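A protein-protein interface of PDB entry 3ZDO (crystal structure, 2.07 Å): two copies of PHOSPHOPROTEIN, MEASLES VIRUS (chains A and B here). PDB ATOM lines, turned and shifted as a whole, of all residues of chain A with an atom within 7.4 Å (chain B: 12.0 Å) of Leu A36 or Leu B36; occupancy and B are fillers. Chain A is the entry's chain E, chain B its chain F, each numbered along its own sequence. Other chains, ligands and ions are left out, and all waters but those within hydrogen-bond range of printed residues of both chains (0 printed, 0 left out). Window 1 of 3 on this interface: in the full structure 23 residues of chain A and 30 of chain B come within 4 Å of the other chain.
NZ of Lys A32 lies within salt-bridge range of OE2 of Glu B34 (2.9 Å).
The side-chain carboxylate (OE2) of Glu B44 is in salt-bridge range of the side-chain amino group (NZ) of Lys B40 (3.4 Å).
Leu B37 touches Lys A32 (CD1 to O, 3.7 Å). Leu B37 touches Ser A35 (CD2 to CB, 3.6 Å). CE of Lys B40 touches O of Ser A35, 3.3 Å away. Leu A36 touches Leu B33 (CD2 to CD2, 3.9 Å). Leu A36 touches Leu B36 (CD1 to CB, 3.5 Å). N of Leu A36 touches CD2 of Leu B37, 3.5 Å away. CD of Lys B40 touches CB of Leu A38, 3.98 Å away. N of Leu A39 touches CD of Lys B40, 3.8 Å away. Leu A39 touches Val B43 (CD1 to CG2, 3.8 Å). Glu A42 touches Glu B44 (OE1 to CG, 3.5 Å).
Of chain B, only Leu B33 (3.9 Å), Leu B36 (3.5 Å) and Leu B37 (3.5 Å) come within 4 Å of Leu A36. Leu B36 touches one residue of chain A. No residue of chain B comes within 4 Å of Leu A33. No residue of chain B comes within 4 Å of Leu A37. Leu A38 touches just one residue of chain B: Lys B40 (3.98 Å). Of the printed residues of chain A, Leu B37 touches Lys A32 (3.7 Å), Ser A35 (3.6 Å) and Leu A36 (3.5 Å). Of the printed residues of chain B, Lys A32 touches Glu B34 and Leu B37. Ile B29 touches none of the printed residues of chain A. The nearest residue of chain A that does not touch Leu B36 is Leu A39 (5.6 Å). The nearest printed residue of chain B that does not touch Glu A42 is Val B43 (4.1 Å).
Printed residues of chain B that touch a printed residue of chain A: Leu B33, Glu B34, Leu B36, Leu B37, Lys B40, Val B43 and Glu B44. Hydrophobic or aromatic side chains of chain B that line the printed part of chain A: Leu B33, Leu B36, Leu B37 and Val B43. Among the printed residues, Asp or Glu carboxylates within 4 Å of a Lys or Arg side-chain nitrogen of the other chain: Lys A32 with Glu B34.
Lys A32 touches Glu B34, but with the chains exchanged Glu A34 does not touch Lys B32 (11.5 Å). Lys A32 touches Leu B37, but with the chains exchanged Leu A37 does not touch Lys B32 (11.2 Å). Ser A35 touches Lys B40, but with the chains exchanged Lys A40 does not touch Ser B35 (13.3 Å). Leu A38 touches Lys B40, but with the chains exchanged Lys A40 does not touch Leu B38 (12.4 Å). Of the 11 pairs that touch across the chains among the printed residues, 1 has its exchanged pair printed and touching as well.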
ATOM      1  N   ILE A  30      17.720 -29.273   9.484  1.00  0.00           N
ATOM      2  CA  ILE A  30      17.521 -30.434   8.594  1.00  0.00           C
ATOM      3  C   ILE A  30      16.535 -30.139   7.456  1.00  0.00           C
ATOM      4  O   ILE A  30      16.869 -30.333   6.269  1.00  0.00           O
ATOM      5  CB  ILE A  30      17.205 -31.767   9.343  1.00  0.00           C
ATOM      6  CG1 ILE A  30      18.497 -32.342   9.961  1.00  0.00           C
ATOM      7  CG2 ILE A  30      16.693 -32.801   8.345  1.00  0.00           C
ATOM      8  CD1 ILE A  30      18.324 -33.153  11.264  1.00  0.00           C
ATOM      9  N   SER A  31      15.350 -29.630   7.810  1.00  0.00           N
ATOM     10  CA  SER A  31      14.300 -29.329   6.836  1.00  0.00           C
ATOM     11  C   SER A  31      14.734 -28.272   5.787  1.00  0.00           C
ATOM     12  O   SER A  31      14.357 -28.374   4.602  1.00  0.00           O
ATOM     13  CB  SER A  31      13.076 -28.803   7.556  1.00  0.00           C
ATOM     14  OG  SER A  31      12.944 -29.478   8.791  1.00  0.00           O
ATOM     15  N   LYS A  32      15.480 -27.260   6.228  1.00  0.00           N
ATOM     16  CA  LYS A  32      15.963 -26.194   5.331  1.00  0.00           C
ATOM     17  C   LYS A  32      17.006 -26.700   4.355  1.00  0.00           C
ATOM     18  O   LYS A  32      17.077 -26.247   3.210  1.00  0.00           O
ATOM     19  CB  LYS A  32      16.618 -25.078   6.131  1.00  0.00           C
ATOM     20  CG  LYS A  32      15.749 -24.469   7.229  1.00  0.00           C
ATOM     21  CD  LYS A  32      14.658 -23.598   6.665  1.00  0.00           C
ATOM     22  CE  LYS A  32      14.161 -22.675   7.779  1.00  0.00           C
ATOM     23  NZ  LYS A  32      13.245 -21.667   7.214  1.00  0.00           N
ATOM     24  N   LEU A  33      17.890 -27.547   4.878  1.00  0.00           N
ATOM     25  CA  LEU A  33      18.991 -28.140   4.154  1.00  0.00           C
ATOM     26  C   LEU A  33      18.448 -29.087   3.067  1.00  0.00           C
ATOM     27  O   LEU A  33      18.923 -29.100   1.925  1.00  0.00           O
ATOM     28  CB  LEU A  33      19.917 -28.888   5.141  1.00  0.00           C
ATOM     29  CG  LEU A  33      21.055 -29.751   4.601  1.00  0.00           C
ATOM     30  CD1 LEU A  33      21.810 -28.938   3.547  1.00  0.00           C
ATOM     31  CD2 LEU A  33      21.978 -30.180   5.753  1.00  0.00           C
ATOM     32  N   GLU A  34      17.406 -29.812   3.421  1.00  0.00           N
ATOM     33  CA  GLU A  34      16.726 -30.694   2.467  1.00  0.00           C
ATOM     34  C   GLU A  34      16.183 -29.912   1.298  1.00  0.00           C
ATOM     35  O   GLU A  34      16.272 -30.340   0.155  1.00  0.00           O
ATOM     36  CB  GLU A  34      15.567 -31.416   3.162  1.00  0.00           C
ATOM     37  CG  GLU A  34      15.992 -32.204   4.387  1.00  0.00           C
ATOM     38  CD  GLU A  34      16.164 -33.686   4.122  1.00  0.00           C
ATOM     39  OE1 GLU A  34      16.593 -34.055   2.995  1.00  0.00           O
ATOM     40  OE2 GLU A  34      15.865 -34.477   5.051  1.00  0.00           O
ATOM     41  N   SER A  35      15.565 -28.783   1.591  1.00  0.00           N
ATOM     42  CA  SER A  35      15.041 -27.889   0.564  1.00  0.00           C
ATOM     43  C   SER A  35      16.155 -27.313  -0.302  1.00  0.00           C
ATOM     44  O   SER A  35      16.029 -27.265  -1.556  1.00  0.00           O
ATOM     45  CB  SER A  35      14.247 -26.741   1.226  1.00  0.00           C
ATOM     46  OG  SER A  35      12.957 -27.162   1.587  1.00  0.00           O
ATOM     47  N   LEU A  36      17.274 -26.956   0.347  1.00  0.00           N
ATOM     48  CA  LEU A  36      18.415 -26.392  -0.357  1.00  0.00           C
ATOM     49  C   LEU A  36      19.018 -27.378  -1.351  1.00  0.00           C
ATOM     50  O   LEU A  36      19.479 -26.986  -2.421  1.00  0.00           O
ATOM     51  CB  LEU A  36      19.499 -25.890   0.633  1.00  0.00           C
ATOM     52  CG  LEU A  36      20.623 -24.993   0.099  1.00  0.00           C
ATOM     53  CD1 LEU A  36      20.149 -23.642  -0.513  1.00  0.00           C
ATOM     54  CD2 LEU A  36      21.590 -24.735   1.259  1.00  0.00           C
ATOM     55  N   LEU A  37      19.020 -28.659  -0.993  1.00  0.00           N
ATOM     56  CA  LEU A  37      19.578 -29.675  -1.861  1.00  0.00           C
ATOM     57  C   LEU A  37      18.881 -29.681  -3.221  1.00  0.00           C
ATOM     58  O   LEU A  37      19.472 -30.072  -4.198  1.00  0.00           O
ATOM     59  CB  LEU A  37      19.474 -31.072  -1.199  1.00  0.00           C
ATOM     60  CG  LEU A  37      20.423 -31.369  -0.054  1.00  0.00           C
ATOM     61  CD1 LEU A  37      20.292 -32.847   0.332  1.00  0.00           C
ATOM     62  CD2 LEU A  37      21.854 -31.058  -0.487  1.00  0.00           C
ATOM     63  N   LEU A  38      17.648 -29.197  -3.308  1.00  0.00           N
ATOM     64  CA  LEU A  38      17.018 -29.038  -4.634  1.00  0.00           C
ATOM     65  C   LEU A  38      17.822 -28.160  -5.611  1.00  0.00           C
ATOM     66  O   LEU A  38      17.669 -28.300  -6.827  1.00  0.00           O
ATOM     67  CB  LEU A  38      15.587 -28.528  -4.544  1.00  0.00           C
ATOM     68  CG  LEU A  38      14.563 -29.502  -3.972  1.00  0.00           C
ATOM     69  CD1 LEU A  38      13.231 -28.777  -3.953  1.00  0.00           C
ATOM     70  CD2 LEU A  38      14.483 -30.730  -4.873  1.00  0.00           C
ATOM     71  N   LEU A  39      18.749 -27.343  -5.090  1.00  0.00           N
ATOM     72  CA  LEU A  39      19.522 -26.413  -5.933  1.00  0.00           C
ATOM     73  C   LEU A  39      20.432 -27.126  -6.938  1.00  0.00           C
ATOM     74  O   LEU A  39      20.719 -26.593  -8.008  1.00  0.00           O
ATOM     75  CB  LEU A  39      20.340 -25.457  -5.009  1.00  0.00           C
ATOM     76  CG  LEU A  39      21.343 -24.459  -5.629  1.00  0.00           C
ATOM     77  CD1 LEU A  39      20.716 -23.340  -6.449  1.00  0.00           C
ATOM     78  CD2 LEU A  39      22.263 -23.910  -4.570  1.00  0.00           C
ATOM     79  N   LYS A  40      20.917 -28.323  -6.581  1.00  0.00           N
ATOM     80  CA  LYS A  40      21.825 -29.068  -7.435  1.00  0.00           C
ATOM     81  C   LYS A  40      21.151 -29.395  -8.718  1.00  0.00           C
ATOM     82  O   LYS A  40      21.740 -29.228  -9.765  1.00  0.00           O
ATOM     83  CB  LYS A  40      22.302 -30.376  -6.785  1.00  0.00           C
ATOM     84  CG  LYS A  40      23.543 -30.213  -5.935  1.00  0.00           C
ATOM     85  CD  LYS A  40      23.262 -30.431  -4.453  1.00  0.00           C
ATOM     86  CE  LYS A  40      23.961 -31.687  -3.960  1.00  0.00           C
ATOM     87  NZ  LYS A  40      23.435 -32.857  -4.723  1.00  0.00           N
ATOM     88  N   GLY A  41      19.884 -29.815  -8.629  1.00  0.00           N
ATOM     89  CA  GLY A  41      19.056 -30.064  -9.819  1.00  0.00           C
ATOM     90  C   GLY A  41      18.651 -28.848 -10.638  1.00  0.00           C
ATOM     91  O   GLY A  41      18.733 -28.859 -11.885  1.00  0.00           O
ATOM     92  N   GLU A  42      18.269 -27.761  -9.979  1.00  0.00           N
ATOM     93  CA  GLU A  42      18.193 -26.435 -10.698  1.00  0.00           C
ATOM     94  C   GLU A  42      19.478 -26.020 -11.478  1.00  0.00           C
ATOM     95  O   GLU A  42      19.419 -25.581 -12.630  1.00  0.00           O
ATOM     96  CB  GLU A  42      17.755 -25.314  -9.726  1.00  0.00           C
ATOM     97  CG  GLU A  42      16.556 -25.719  -8.844  1.00  0.00           C
ATOM     98  CD  GLU A  42      15.290 -26.012  -9.685  1.00  0.00           C
ATOM     99  OE1 GLU A  42      15.043 -25.291 -10.659  1.00  0.00           O
ATOM    100  OE2 GLU A  42      14.519 -26.942  -9.365  1.00  0.00           O
ATOM    101  N   ASN B  26      22.885 -21.534  16.260  1.00  0.00           N
ATOM    102  CA  ASN B  26      21.889 -22.274  15.438  1.00  0.00           C
ATOM    103  C   ASN B  26      20.947 -21.327  14.726  1.00  0.00           C
ATOM    104  O   ASN B  26      20.646 -21.518  13.572  1.00  0.00           O
ATOM    105  CB  ASN B  26      21.083 -23.292  16.285  1.00  0.00           C
ATOM    106  CG  ASN B  26      21.848 -24.576  16.562  1.00  0.00           C
ATOM    107  OD1 ASN B  26      21.496 -25.333  17.479  1.00  0.00           O
ATOM    108  ND2 ASN B  26      22.892 -24.838  15.778  1.00  0.00           N
ATOM    109  N   GLN B  27      20.559 -20.238  15.392  1.00  0.00           N
ATOM    110  CA  GLN B  27      19.777 -19.172  14.747  1.00  0.00           C
ATOM    111  C   GLN B  27      20.492 -18.456  13.586  1.00  0.00           C
ATOM    112  O   GLN B  27      19.841 -18.100  12.593  1.00  0.00           O
ATOM    113  CB  GLN B  27      19.259 -18.154  15.779  1.00  0.00           C
ATOM    114  CG  GLN B  27      18.624 -18.794  16.991  1.00  0.00           C
ATOM    115  CD  GLN B  27      17.611 -19.848  16.605  1.00  0.00           C
ATOM    116  OE1 GLN B  27      16.746 -19.626  15.750  1.00  0.00           O
ATOM    117  NE2 GLN B  27      17.706 -21.014  17.241  1.00  0.00           N
ATOM    118  N   LYS B  28      21.794 -18.212  13.727  1.00  0.00           N
ATOM    119  CA  LYS B  28      22.585 -17.617  12.638  1.00  0.00           C
ATOM    120  C   LYS B  28      22.749 -18.645  11.482  1.00  0.00           C
ATOM    121  O   LYS B  28      22.675 -18.275  10.359  1.00  0.00           O
ATOM    122  CB  LYS B  28      23.968 -17.171  13.197  1.00  0.00           C
ATOM    123  CG  LYS B  28      25.005 -16.690  12.198  1.00  0.00           C
ATOM    124  CD  LYS B  28      26.371 -16.472  12.865  1.00  0.00           C
ATOM    125  CE  LYS B  28      27.532 -16.758  11.905  1.00  0.00           C
ATOM    126  NZ  LYS B  28      28.882 -16.265  12.343  1.00  0.00           N
ATOM    127  N   ILE B  29      22.990 -19.928  11.790  1.00  0.00           N
ATOM    128  CA  ILE B  29      23.114 -20.967  10.747  1.00  0.00           C
ATOM    129  C   ILE B  29      21.783 -21.005   9.995  1.00  0.00           C
ATOM    130  O   ILE B  29      21.753 -21.033   8.786  1.00  0.00           O
ATOM    131  CB  ILE B  29      23.413 -22.381  11.365  1.00  0.00           C
ATOM    132  CG1 ILE B  29      24.879 -22.410  11.746  1.00  0.00           C
ATOM    133  CG2 ILE B  29      23.090 -23.482  10.336  1.00  0.00           C
ATOM    134  CD1 ILE B  29      25.410 -23.584  12.536  1.00  0.00           C
ATOM    135  N   ILE B  30      20.678 -20.850  10.724  1.00  0.00           N
ATOM    136  CA  ILE B  30      19.319 -20.926  10.126  1.00  0.00           C
ATOM    137  C   ILE B  30      19.033 -19.729   9.210  1.00  0.00           C
ATOM    138  O   ILE B  30      18.446 -19.890   8.144  1.00  0.00           O
ATOM    139  CB  ILE B  30      18.188 -20.993  11.209  1.00  0.00           C
ATOM    140  CG1 ILE B  30      18.242 -22.336  11.923  1.00  0.00           C
ATOM    141  CG2 ILE B  30      16.812 -20.805  10.554  1.00  0.00           C
ATOM    142  CD1 ILE B  30      17.316 -22.473  13.113  1.00  0.00           C
ATOM    143  N   SER B  31      19.459 -18.534   9.623  1.00  0.00           N
ATOM    144  CA  SER B  31      19.384 -17.374   8.739  1.00  0.00           C
ATOM    145  C   SER B  31      20.155 -17.570   7.433  1.00  0.00           C
ATOM    146  O   SER B  31      19.673 -17.178   6.358  1.00  0.00           O
ATOM    147  CB  SER B  31      19.920 -16.141   9.423  1.00  0.00           C
ATOM    148  OG  SER B  31      18.932 -15.656  10.280  1.00  0.00           O
ATOM    149  N   LYS B  32      21.362 -18.133   7.530  1.00  0.00           N
ATOM    150  CA  LYS B  32      22.220 -18.256   6.328  1.00  0.00           C
ATOM    151  C   LYS B  32      21.575 -19.253   5.405  1.00  0.00           C
ATOM    152  O   LYS B  32      21.626 -19.081   4.184  1.00  0.00           O
ATOM    153  CB  LYS B  32      23.640 -18.694   6.675  1.00  0.00           C
ATOM    154  CG  LYS B  32      24.419 -17.659   7.439  1.00  0.00           C
ATOM    155  CD  LYS B  32      25.646 -18.310   8.047  1.00  0.00           C
ATOM    156  CE  LYS B  32      26.278 -17.408   9.090  1.00  0.00           C
ATOM    157  NZ  LYS B  32      26.657 -16.069   8.578  1.00  0.00           N
ATOM    158  N   LEU B  33      20.981 -20.309   5.980  1.00  0.00           N
ATOM    159  CA  LEU B  33      20.231 -21.288   5.173  1.00  0.00           C
ATOM    160  C   LEU B  33      19.056 -20.627   4.456  1.00  0.00           C
ATOM    161  O   LEU B  33      18.860 -20.843   3.251  1.00  0.00           O
ATOM    162  CB  LEU B  33      19.752 -22.483   6.002  1.00  0.00           C
ATOM    163  CG  LEU B  33      20.855 -23.518   6.350  1.00  0.00           C
ATOM    164  CD1 LEU B  33      20.388 -24.491   7.419  1.00  0.00           C
ATOM    165  CD2 LEU B  33      21.341 -24.265   5.093  1.00  0.00           C
ATOM    166  N   GLU B  34      18.278 -19.837   5.206  1.00  0.00           N
ATOM    167  CA  GLU B  34      17.176 -19.021   4.638  1.00  0.00           C
ATOM    168  C   GLU B  34      17.555 -18.114   3.421  1.00  0.00           C
ATOM    169  O   GLU B  34      16.834 -18.055   2.402  1.00  0.00           O
ATOM    170  CB  GLU B  34      16.449 -18.233   5.750  1.00  0.00           C
ATOM    171  CG  GLU B  34      15.708 -19.206   6.670  1.00  0.00           C
ATOM    172  CD  GLU B  34      15.006 -18.550   7.860  1.00  0.00           C
ATOM    173  OE1 GLU B  34      15.196 -17.338   8.066  1.00  0.00           O
ATOM    174  OE2 GLU B  34      14.173 -19.232   8.524  1.00  0.00           O
ATOM    175  N   SER B  35      18.673 -17.432   3.556  1.00  0.00           N
ATOM    176  CA  SER B  35      19.228 -16.571   2.538  1.00  0.00           C
ATOM    177  C   SER B  35      19.665 -17.412   1.270  1.00  0.00           C
ATOM    178  O   SER B  35      19.489 -16.978   0.150  1.00  0.00           O
ATOM    179  CB  SER B  35      20.443 -15.857   3.176  1.00  0.00           C
ATOM    180  OG  SER B  35      21.252 -15.205   2.199  1.00  0.00           O
ATOM    181  N   LEU B  36      20.244 -18.590   1.478  1.00  0.00           N
ATOM    182  CA  LEU B  36      20.509 -19.538   0.381  1.00  0.00           C
ATOM    183  C   LEU B  36      19.241 -20.072  -0.301  1.00  0.00           C
ATOM    184  O   LEU B  36      19.206 -20.348  -1.542  1.00  0.00           O
ATOM    185  CB  LEU B  36      21.408 -20.709   0.906  1.00  0.00           C
ATOM    186  CG  LEU B  36      22.864 -20.230   1.182  1.00  0.00           C
ATOM    187  CD1 LEU B  36      23.630 -21.233   2.045  1.00  0.00           C
ATOM    188  CD2 LEU B  36      23.681 -19.865  -0.118  1.00  0.00           C
ATOM    189  N   LEU B  37      18.215 -20.278   0.493  1.00  0.00           N
ATOM    190  CA  LEU B  37      16.936 -20.685  -0.080  1.00  0.00           C
ATOM    191  C   LEU B  37      16.298 -19.598  -0.958  1.00  0.00           C
ATOM    192  O   LEU B  37      15.736 -19.911  -2.028  1.00  0.00           O
ATOM    193  CB  LEU B  37      15.965 -21.217   1.016  1.00  0.00           C
ATOM    194  CG  LEU B  37      16.311 -22.618   1.574  1.00  0.00           C
ATOM    195  CD1 LEU B  37      15.505 -22.960   2.849  1.00  0.00           C
ATOM    196  CD2 LEU B  37      16.059 -23.699   0.551  1.00  0.00           C
ATOM    197  N   LEU B  38      16.480 -18.317  -0.584  1.00  0.00           N
ATOM    198  CA  LEU B  38      16.052 -17.240  -1.477  1.00  0.00           C
ATOM    199  C   LEU B  38      16.870 -17.283  -2.774  1.00  0.00           C
ATOM    200  O   LEU B  38      16.339 -17.003  -3.877  1.00  0.00           O
ATOM    201  CB  LEU B  38      16.233 -15.845  -0.822  1.00  0.00           C
ATOM    202  CG  LEU B  38      15.463 -15.581   0.478  1.00  0.00           C
ATOM    203  CD1 LEU B  38      15.845 -14.180   1.011  1.00  0.00           C
ATOM    204  CD2 LEU B  38      13.984 -15.636   0.164  1.00  0.00           C
ATOM    205  N   LEU B  39      18.153 -17.623  -2.650  1.00  0.00           N
ATOM    206  CA  LEU B  39      19.027 -17.605  -3.850  1.00  0.00           C
ATOM    207  C   LEU B  39      18.583 -18.737  -4.777  1.00  0.00           C
ATOM    208  O   LEU B  39      18.618 -18.588  -5.984  1.00  0.00           O
ATOM    209  CB  LEU B  39      20.512 -17.667  -3.477  1.00  0.00           C
ATOM    210  CG  LEU B  39      21.529 -18.067  -4.573  1.00  0.00           C
ATOM    211  CD1 LEU B  39      22.844 -17.375  -4.306  1.00  0.00           C
ATOM    212  CD2 LEU B  39      21.774 -19.583  -4.585  1.00  0.00           C
ATOM    213  N   LYS B  40      18.082 -19.838  -4.191  1.00  0.00           N
ATOM    214  CA  LYS B  40      17.441 -20.930  -4.975  1.00  0.00           C
ATOM    215  C   LYS B  40      16.250 -20.470  -5.844  1.00  0.00           C
ATOM    216  O   LYS B  40      16.214 -20.762  -7.030  1.00  0.00           O
ATOM    217  CB  LYS B  40      17.110 -22.193  -4.112  1.00  0.00           C
ATOM    218  CG  LYS B  40      16.571 -23.391  -4.929  1.00  0.00           C
ATOM    219  CD  LYS B  40      16.336 -24.648  -4.089  1.00  0.00           C
ATOM    220  CE  LYS B  40      15.078 -24.536  -3.210  1.00  0.00           C
ATOM    221  NZ  LYS B  40      13.837 -24.425  -4.025  1.00  0.00           N
ATOM    222  N   GLY B  41      15.344 -19.672  -5.290  1.00  0.00           N
ATOM    223  CA  GLY B  41      14.335 -18.888  -6.084  1.00  0.00           C
ATOM    224  C   GLY B  41      14.856 -18.102  -7.306  1.00  0.00           C
ATOM    225  O   GLY B  41      14.271 -18.143  -8.417  1.00  0.00           O
ATOM    226  N   GLU B  42      15.943 -17.359  -7.126  1.00  0.00           N
ATOM    227  CA  GLU B  42      16.586 -16.665  -8.285  1.00  0.00           C
ATOM    228  C   GLU B  42      17.217 -17.589  -9.343  1.00  0.00           C
ATOM    229  O   GLU B  42      17.196 -17.281 -10.562  1.00  0.00           O
ATOM    230  CB  GLU B  42      17.645 -15.676  -7.757  1.00  0.00           C
ATOM    231  CG  GLU B  42      17.058 -14.610  -6.826  1.00  0.00           C
ATOM    232  CD  GLU B  42      18.094 -13.583  -6.386  1.00  0.00           C
ATOM    233  OE1 GLU B  42      18.661 -12.885  -7.251  1.00  0.00           O
ATOM    234  OE2 GLU B  42      18.344 -13.469  -5.180  1.00  0.00           O
ATOM    235  N   VAL B  43      17.824 -18.688  -8.880  1.00  0.00           N
ATOM    236  CA  VAL B  43      18.431 -19.694  -9.774  1.00  0.00           C
ATOM    237  C   VAL B  43      17.279 -20.323 -10.571  1.00  0.00           C
ATOM    238  O   VAL B  43      17.373 -20.494 -11.816  1.00  0.00           O
ATOM    239  CB  VAL B  43      19.352 -20.739  -9.018  1.00  0.00           C
ATOM    240  CG1 VAL B  43      19.915 -21.840  -9.965  1.00  0.00           C
ATOM    241  CG2 VAL B  43      20.581 -20.044  -8.405  1.00  0.00           C
ATOM    242  N   GLU B  44      16.166 -20.609  -9.890  1.00  0.00           N
ATOM    243  CA  GLU B  44      14.922 -21.030 -10.612  1.00  0.00           C
ATOM    244  C   GLU B  44      14.458 -20.088 -11.680  1.00  0.00           C
ATOM    245  O   GLU B  44      14.079 -20.529 -12.752  1.00  0.00           O
ATOM    246  CB  GLU B  44      13.735 -21.239  -9.669  1.00  0.00           C
ATOM    247  CG  GLU B  44      13.775 -22.549  -8.949  1.00  0.00           C
ATOM    248  CD  GLU B  44      12.620 -22.691  -7.978  1.00  0.00           C
ATOM    249  OE1 GLU B  44      11.472 -22.884  -8.440  1.00  0.00           O
ATOM    250  OE2 GLU B  44      12.875 -22.632  -6.758  1.00  0.00           O
ATOM    251  N   SER B  45      14.488 -18.782 -11.406  1.00  0.00           N
ATOM    252  CA  SER B  45      14.132 -17.795 -12.430  1.00  0.00           C
ATOM    253  C   SER B  45      15.147 -17.786 -13.590  1.00  0.00           C
ATOM    254  O   SER B  45      14.767 -17.672 -14.753  1.00  0.00           O
ATOM    255  CB  SER B  45      13.982 -16.392 -11.812  1.00  0.00           C
ATOM    256  OG  SER B  45      12.993 -16.392 -10.810  1.00  0.00           O
ATOM    257  N   ILE B  46      16.430 -17.904 -13.266  1.00  0.00           N
ATOM    258  CA  ILE B  46      17.480 -17.996 -14.301  1.00  0.00           C
ATOM    259  C   ILE B  46      17.190 -19.177 -15.235  1.00  0.00           C
ATOM    260  O   ILE B  46      17.096 -18.967 -16.422  1.00  0.00           O
ATOM    261  CB  ILE B  46      18.910 -18.124 -13.715  1.00  0.00           C
ATOM    262  CG1 ILE B  46      19.321 -16.833 -13.024  1.00  0.00           C
ATOM    263  CG2 ILE B  46      19.957 -18.462 -14.812  1.00  0.00           C
ATOM    264  CD1 ILE B  46      20.502 -17.035 -12.095  1.00  0.00           C
